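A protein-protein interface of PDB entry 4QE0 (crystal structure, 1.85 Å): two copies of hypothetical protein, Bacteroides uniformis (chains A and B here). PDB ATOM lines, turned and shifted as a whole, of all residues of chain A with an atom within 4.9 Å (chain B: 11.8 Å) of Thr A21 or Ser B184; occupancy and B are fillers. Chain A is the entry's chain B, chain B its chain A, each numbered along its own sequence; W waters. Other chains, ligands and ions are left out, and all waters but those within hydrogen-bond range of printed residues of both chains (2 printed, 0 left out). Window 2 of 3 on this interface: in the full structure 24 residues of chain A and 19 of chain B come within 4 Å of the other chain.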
ATOM      1  N   MLY A  19     -19.154  -9.712 -20.517  1.00  0.00           N
ATOM      2  CA  MLY A  19     -18.557  -8.737 -19.579  1.00  0.00           C
ATOM      3  CB  MLY A  19     -17.829  -9.359 -18.370  1.00  0.00           C
ATOM      4  CG  MLY A  19     -18.246 -10.761 -17.978  1.00  0.00           C
ATOM      5  CD  MLY A  19     -17.244 -11.350 -16.985  1.00  0.00           C
ATOM      6  CE  MLY A  19     -17.402 -10.749 -15.594  1.00  0.00           C
ATOM      7  NZ  MLY A  19     -17.245 -11.817 -14.587  1.00  0.00           N
ATOM      8  CH1 MLY A  19     -15.995 -11.629 -13.832  1.00  0.00           C
ATOM      9  CH2 MLY A  19     -18.393 -11.825 -13.666  1.00  0.00           C
ATOM     10  C   MLY A  19     -17.512  -7.887 -20.236  1.00  0.00           C
ATOM     11  O   MLY A  19     -17.238  -6.772 -19.782  1.00  0.00           O
ATOM     12  N   MLY A  20     -16.890  -8.412 -21.281  1.00  0.00           N
ATOM     13  CA  MLY A  20     -15.821  -7.715 -21.974  1.00  0.00           C
ATOM     14  CB  MLY A  20     -14.479  -7.939 -21.269  1.00  0.00           C
ATOM     15  CG  MLY A  20     -14.029  -9.394 -21.296  1.00  0.00           C
ATOM     16  CD  MLY A  20     -12.772  -9.541 -20.434  1.00  0.00           C
ATOM     17  CE  MLY A  20     -12.069 -10.875 -20.674  1.00  0.00           C
ATOM     18  NZ  MLY A  20     -10.922 -11.039 -19.751  1.00  0.00           N
ATOM     19  CH1 MLY A  20     -10.447 -12.435 -19.799  1.00  0.00           C
ATOM     20  CH2 MLY A  20      -9.814 -10.121 -20.094  1.00  0.00           C
ATOM     21  C   MLY A  20     -15.753  -8.217 -23.392  1.00  0.00           C
ATOM     22  O   MLY A  20     -16.388  -9.203 -23.750  1.00  0.00           O
ATOM     23  N   THR A  21     -14.965  -7.537 -24.209  1.00  0.00           N
ATOM     24  CA  THR A  21     -14.846  -7.892 -25.600  1.00  0.00           C
ATOM     25  C   THR A  21     -14.304  -9.319 -25.718  1.00  0.00           C
ATOM     26  O   THR A  21     -13.256  -9.632 -25.161  1.00  0.00           O
ATOM     27  CB  THR A  21     -13.974  -6.876 -26.325  1.00  0.00           C
ATOM     28  OG1 THR A  21     -14.634  -5.597 -26.280  1.00  0.00           O
ATOM     29  CG2 THR A  21     -13.753  -7.278 -27.759  1.00  0.00           C
ATOM     30  N   THR A  22     -15.037 -10.169 -26.423  1.00  0.00           N
ATOM     31  CA  THR A  22     -14.783 -11.619 -26.432  1.00  0.00           C
ATOM     32  C   THR A  22     -15.325 -12.223 -27.728  1.00  0.00           C
ATOM     33  O   THR A  22     -16.300 -11.732 -28.288  1.00  0.00           O
ATOM     34  CB  THR A  22     -15.551 -12.349 -25.294  1.00  0.00           C
ATOM     35  OG1 THR A  22     -15.432 -11.650 -24.042  1.00  0.00           O
ATOM     36  CG2 THR A  22     -15.047 -13.786 -25.133  1.00  0.00           C
ATOM     37  N   THR A  23     -14.712 -13.308 -28.180  1.00  0.00           N
ATOM     38  CA  THR A  23     -15.257 -14.093 -29.276  1.00  0.00           C
ATOM     39  C   THR A  23     -15.779 -15.396 -28.701  1.00  0.00           C
ATOM     40  O   THR A  23     -15.085 -16.051 -27.917  1.00  0.00           O
ATOM     41  CB  THR A  23     -14.185 -14.344 -30.326  1.00  0.00           C
ATOM     42  OG1 THR A  23     -13.659 -13.081 -30.728  1.00  0.00           O
ATOM     43  CG2 THR A  23     -14.752 -15.054 -31.518  1.00  0.00           C
ATOM     44  N   GLN A  32     -19.309 -12.481 -31.949  1.00  0.00           N
ATOM     45  CA  GLN A  32     -18.428 -11.498 -31.405  1.00  0.00           C
ATOM     46  C   GLN A  32     -19.219 -10.667 -30.400  1.00  0.00           C
ATOM     47  O   GLN A  32     -20.351 -10.257 -30.656  1.00  0.00           O
ATOM     48  CB  GLN A  32     -17.909 -10.597 -32.514  1.00  0.00           C
ATOM     49  CG  GLN A  32     -16.939  -9.527 -32.037  1.00  0.00           C
ATOM     50  CD  GLN A  32     -15.707 -10.132 -31.391  1.00  0.00           C
ATOM     51  OE1 GLN A  32     -15.227 -11.174 -31.825  1.00  0.00           O
ATOM     52  NE2 GLN A  32     -15.196  -9.487 -30.354  1.00  0.00           N
ATOM     53  N   CYS A  33     -18.597 -10.430 -29.260  1.00  0.00           N
ATOM     54  CA  CYS A  33     -19.153  -9.594 -28.217  1.00  0.00           C
ATOM     55  C   CYS A  33     -18.201  -8.424 -28.057  1.00  0.00           C
ATOM     56  O   CYS A  33     -17.057  -8.606 -27.625  1.00  0.00           O
ATOM     57  CB  CYS A  33     -19.267 -10.436 -26.956  1.00  0.00           C
ATOM     58  SG  CYS A  33     -19.609  -9.559 -25.426  1.00  0.00           S
ATOM     59  N   ASP A  34     -18.632  -7.231 -28.467  1.00  0.00           N
ATOM     60  CA  ASP A  34     -17.824  -6.020 -28.314  1.00  0.00           C
ATOM     61  C   ASP A  34     -18.378  -5.234 -27.144  1.00  0.00           C
ATOM     62  O   ASP A  34     -19.563  -4.929 -27.110  1.00  0.00           O
ATOM     63  CB  ASP A  34     -17.869  -5.153 -29.567  1.00  0.00           C
ATOM     64  CG  ASP A  34     -17.071  -5.737 -30.723  1.00  0.00           C
ATOM     65  OD1 ASP A  34     -16.193  -6.588 -30.493  1.00  0.00           O
ATOM     66  OD2 ASP A  34     -17.298  -5.319 -31.865  1.00  0.00           O
ATOM     67  N   VAL A  35     -17.524  -4.913 -26.176  1.00  0.00           N
ATOM     68  CA  VAL A  35     -17.971  -4.161 -25.004  1.00  0.00           C
ATOM     69  C   VAL A  35     -17.144  -2.899 -24.882  1.00  0.00           C
ATOM     70  O   VAL A  35     -15.912  -2.950 -24.849  1.00  0.00           O
ATOM     71  CB  VAL A  35     -17.837  -4.952 -23.711  1.00  0.00           C
ATOM     72  CG1 VAL A  35     -18.345  -4.136 -22.530  1.00  0.00           C
ATOM     73  CG2 VAL A  35     -18.580  -6.263 -23.821  1.00  0.00           C
ATOM     74  N   ASP A  36     -17.831  -1.765 -24.820  1.00  0.00           N
ATOM     75  CA  ASP A  36     -17.173  -0.493 -24.574  1.00  0.00           C
ATOM     76  C   ASP A  36     -17.002  -0.366 -23.073  1.00  0.00           C
ATOM     77  O   ASP A  36     -17.984  -0.338 -22.335  1.00  0.00           O
ATOM     78  CB  ASP A  36     -18.009   0.663 -25.104  1.00  0.00           C
ATOM     79  CG  ASP A  36     -17.397   2.023 -24.778  1.00  0.00           C
ATOM     80  OD1 ASP A  36     -16.222   2.246 -25.132  1.00  0.00           O
ATOM     81  OD2 ASP A  36     -18.099   2.866 -24.180  1.00  0.00           O
ATOM     82  N   ASP A  37     -15.760  -0.290 -22.613  1.00  0.00           N
ATOM     83  CA  ASP A  37     -15.506  -0.339 -21.176  1.00  0.00           C
ATOM     84  C   ASP A  37     -16.127   0.838 -20.414  1.00  0.00           C
ATOM     85  O   ASP A  37     -16.708   0.632 -19.350  1.00  0.00           O
ATOM     86  CB  ASP A  37     -14.011  -0.480 -20.888  1.00  0.00           C
ATOM     87  CG  ASP A  37     -13.499  -1.911 -21.118  1.00  0.00           C
ATOM     88  OD1 ASP A  37     -14.311  -2.867 -21.262  1.00  0.00           O
ATOM     89  OD2 ASP A  37     -12.266  -2.082 -21.162  1.00  0.00           O
ATOM     90  N   ASP B  77     -17.905  12.561 -25.043  1.00  0.00           N
ATOM     91  CA  ASP B  77     -18.067  11.175 -25.442  1.00  0.00           C
ATOM     92  C   ASP B  77     -19.181  11.104 -26.456  1.00  0.00           C
ATOM     93  O   ASP B  77     -20.333  11.381 -26.138  1.00  0.00           O
ATOM     94  CB  ASP B  77     -18.381  10.269 -24.254  1.00  0.00           C
ATOM     95  CG  ASP B  77     -18.306   8.786 -24.646  1.00  0.00           C
ATOM     96  OD1 ASP B  77     -19.251   8.234 -25.235  1.00  0.00           O
ATOM     97  OD2 ASP B  77     -17.231   8.168 -24.471  1.00  0.00           O
ATOM     98  N   ARG B  78     -18.829  10.710 -27.667  1.00  0.00           N
ATOM     99  CA  ARG B  78     -19.754  10.733 -28.773  1.00  0.00           C
ATOM    100  C   ARG B  78     -20.940   9.809 -28.515  1.00  0.00           C
ATOM    101  O   ARG B  78     -22.100  10.219 -28.584  1.00  0.00           O
ATOM    102  CB  ARG B  78     -19.030  10.327 -30.069  1.00  0.00           C
ATOM    103  CG  ARG B  78     -19.849  10.544 -31.345  1.00  0.00           C
ATOM    104  CD  ARG B  78     -20.679   9.359 -31.741  1.00  0.00           C
ATOM    105  NE  ARG B  78     -20.001   8.065 -31.701  1.00  0.00           N
ATOM    106  CZ  ARG B  78     -20.654   6.909 -31.764  1.00  0.00           C
ATOM    107  NH1 ARG B  78     -21.968   6.908 -31.912  1.00  0.00           N
ATOM    108  NH2 ARG B  78     -20.006   5.742 -31.700  1.00  0.00           N
ATOM    109  N   PHE B  79     -20.649   8.563 -28.183  1.00  0.00           N
ATOM    110  CA  PHE B  79     -21.703   7.609 -27.954  1.00  0.00           C
ATOM    111  C   PHE B  79     -22.649   8.018 -26.833  1.00  0.00           C
ATOM    112  O   PHE B  79     -23.873   7.931 -26.986  1.00  0.00           O
ATOM    113  CB  PHE B  79     -21.158   6.204 -27.672  1.00  0.00           C
ATOM    114  CG  PHE B  79     -22.260   5.208 -27.390  1.00  0.00           C
ATOM    115  CD1 PHE B  79     -23.170   4.878 -28.365  1.00  0.00           C
ATOM    116  CD2 PHE B  79     -22.433   4.690 -26.114  1.00  0.00           C
ATOM    117  CE1 PHE B  79     -24.214   4.002 -28.109  1.00  0.00           C
ATOM    118  CE2 PHE B  79     -23.486   3.822 -25.839  1.00  0.00           C
ATOM    119  CZ  PHE B  79     -24.372   3.478 -26.835  1.00  0.00           C
ATOM    120  N   MET B  80     -22.101   8.403 -25.693  1.00  0.00           N
ATOM    121  CA  MET B  80     -22.947   8.754 -24.554  1.00  0.00           C
ATOM    122  C   MET B  80     -23.802   9.951 -24.883  1.00  0.00           C
ATOM    123  O   MET B  80     -24.948   9.996 -24.469  1.00  0.00           O
ATOM    124  CB  MET B  80     -22.135   8.984 -23.279  1.00  0.00           C
ATOM    125  CG  MET B  80     -21.505   7.706 -22.752  1.00  0.00           C
ATOM    126  SD  MET B  80     -22.695   6.714 -21.523  1.00  0.00           S
ATOM    127  CE  MET B  80     -23.895   5.665 -22.701  1.00  0.00           C
ATOM    128  N   HIS B 151     -23.480   8.665 -18.503  1.00  0.00           N
ATOM    129  CA  HIS B 151     -22.507   9.328 -17.633  1.00  0.00           C
ATOM    130  C   HIS B 151     -21.426   9.949 -18.473  1.00  0.00           C
ATOM    131  O   HIS B 151     -21.171   9.512 -19.593  1.00  0.00           O
ATOM    132  CB  HIS B 151     -21.919   8.338 -16.633  1.00  0.00           C
ATOM    133  CG  HIS B 151     -21.279   7.159 -17.273  1.00  0.00           C
ATOM    134  ND1 HIS B 151     -19.971   7.169 -17.700  1.00  0.00           N
ATOM    135  CD2 HIS B 151     -21.772   5.938 -17.587  1.00  0.00           C
ATOM    136  CE1 HIS B 151     -19.685   6.008 -18.258  1.00  0.00           C
ATOM    137  NE2 HIS B 151     -20.760   5.243 -18.202  1.00  0.00           N
ATOM    138  N   PRO B 180     -22.764   2.098 -32.483  1.00  0.00           N
ATOM    139  CA  PRO B 180     -22.160   1.736 -31.211  1.00  0.00           C
ATOM    140  C   PRO B 180     -20.698   2.189 -31.134  1.00  0.00           C
ATOM    141  O   PRO B 180     -20.062   2.397 -32.167  1.00  0.00           O
ATOM    142  CB  PRO B 180     -22.277   0.206 -31.169  1.00  0.00           C
ATOM    143  CG  PRO B 180     -22.586  -0.220 -32.547  1.00  0.00           C
ATOM    144  CD  PRO B 180     -23.145   0.941 -33.300  1.00  0.00           C
ATOM    145  N   PRO B 181     -20.173   2.352 -29.924  1.00  0.00           N
ATOM    146  CA  PRO B 181     -18.757   2.644 -29.789  1.00  0.00           C
ATOM    147  C   PRO B 181     -17.955   1.367 -30.158  1.00  0.00           C
ATOM    148  O   PRO B 181     -18.505   0.280 -30.102  1.00  0.00           O
ATOM    149  CB  PRO B 181     -18.617   2.993 -28.312  1.00  0.00           C
ATOM    150  CG  PRO B 181     -19.751   2.310 -27.629  1.00  0.00           C
ATOM    151  CD  PRO B 181     -20.799   1.995 -28.635  1.00  0.00           C
ATOM    152  N   PRO B 182     -16.693   1.501 -30.576  1.00  0.00           N
ATOM    153  CA  PRO B 182     -15.955   0.262 -30.874  1.00  0.00           C
ATOM    154  C   PRO B 182     -15.651  -0.518 -29.587  1.00  0.00           C
ATOM    155  O   PRO B 182     -15.614   0.067 -28.498  1.00  0.00           O
ATOM    156  CB  PRO B 182     -14.673   0.772 -31.533  1.00  0.00           C
ATOM    157  CG  PRO B 182     -14.479   2.141 -30.966  1.00  0.00           C
ATOM    158  CD  PRO B 182     -15.850   2.704 -30.690  1.00  0.00           C
ATOM    159  N   GLY B 183     -15.460  -1.825 -29.701  1.00  0.00           N
ATOM    160  CA  GLY B 183     -15.187  -2.637 -28.522  1.00  0.00           C
ATOM    161  C   GLY B 183     -13.822  -2.286 -27.951  1.00  0.00           C
ATOM    162  O   GLY B 183     -12.870  -2.111 -28.709  1.00  0.00           O
ATOM    163  N   SER B 184     -13.731  -2.172 -26.627  1.00  0.00           N
ATOM    164  CA  SER B 184     -12.445  -1.961 -25.950  1.00  0.00           C
ATOM    165  C   SER B 184     -11.544  -3.190 -26.135  1.00  0.00           C
ATOM    166  O   SER B 184     -12.055  -4.305 -26.299  1.00  0.00           O
ATOM    167  CB  SER B 184     -12.656  -1.699 -24.461  1.00  0.00           C
ATOM    168  OG  SER B 184     -13.441  -0.539 -24.253  1.00  0.00           O
ATOM    169  N   LEU B 185     -10.229  -2.973 -26.095  1.00  0.00           N
ATOM    170  CA  LEU B 185      -9.203  -4.038 -26.236  1.00  0.00           C
ATOM    171  C   LEU B 185      -9.400  -4.881 -27.493  1.00  0.00           C
ATOM    172  O   LEU B 185      -9.176  -4.412 -28.606  1.00  0.00           O
ATOM    173  CB  LEU B 185      -9.161  -4.958 -25.001  1.00  0.00           C
ATOM    174  CG  LEU B 185      -8.255  -4.563 -23.827  1.00  0.00           C
ATOM    175  CD1 LEU B 185      -8.892  -3.485 -22.958  1.00  0.00           C
ATOM    176  CD2 LEU B 185      -7.915  -5.789 -22.984  1.00  0.00           C
HETATM  177  O   HOH W   1     -15.190  -3.308 -32.178  1.00  0.00           O
HETATM  178  O   HOH W   2     -18.898   5.557 -24.213  1.00  0.00           O
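O of Ser B184 is in hydrogen-bond range of OG1 of Thr A21, 2.9 Å away.
N of Ser B184 sits at hydrogen-bond distance from O of Val A35 (2.9 Å).
The side-chain hydroxyl of Ser B184 lies within hydrogen-bond range of the backbone NH of Asp A37.
No position is printed for both chains.
The side-chain hydroxyl (OG1) of Thr A21 is in hydrogen-bond range of the backbone NH (N) of Val A35.
The side-chain amide nitrogen of Gln A32 is in hydrogen-bond range of the side-chain carboxylate of Asp A34.
Among the printed residues, merely in contact across the chains: Asp A36 with Pro B181 (3.5 Å), Asp A36 with Ser B184 (3.7 Å), Thr A21 with Gly B183 (3.8 Å), Val A35 with Gly B183 (3.8 Å) and Asp A34 with Gly B183 (3.8 Å).
MLY A20 touches none of the printed residues of chain B.
Thr A21 touches just these residues of chain B: Gly B183 (3.8 Å) and Ser B184 (2.9 Å).
No residue of chain B comes within 4 Å of Thr A22.
Cys A33 touches none of the printed residues of chain B.
Of chain B, only Gly B183 (3.8 Å) comes within 4 Å of Asp A34.
Of chain B, only Ser B184 (2.9 Å) comes within 4 Å of Asp A37.
Printed residues of chain A within 4 Å of Pro B181: Asp A36.
Pro B182 touches none of the printed residues of chain A.
Of the printed residues of chain A, Gly B183 touches Thr A21 (3.8 Å), Asp A34 (3.8 Å) and Val A35 (3.8 Å).
Of chain A, only Thr A21, Val A35, Asp A36 and Asp A37 come within 4 Å of Ser B184.
The nearest printed residue of chain A that does not touch Pro B181 is Asp A34 (5.5 Å).
Water W2 bridges OD2 of Asp A36 and OD1 of Asp B77.
Water W1 lies within hydrogen-bond range of N of Gly B183 (2.9 Å) and OD2 of Asp A34 (2.9 Å).
Hydrophobic or aromatic side chains of chain B that line the printed part of chain A: Pro B181.
Of the 11 printed residues of chain A, 5 touch a printed residue of chain B.
Among the printed residues, 8 pairs touch across the chains.
Among the printed residues, no Asp or Glu carboxylate lies within 4 Å of a Lys or Arg side-chain nitrogen of the other chain.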
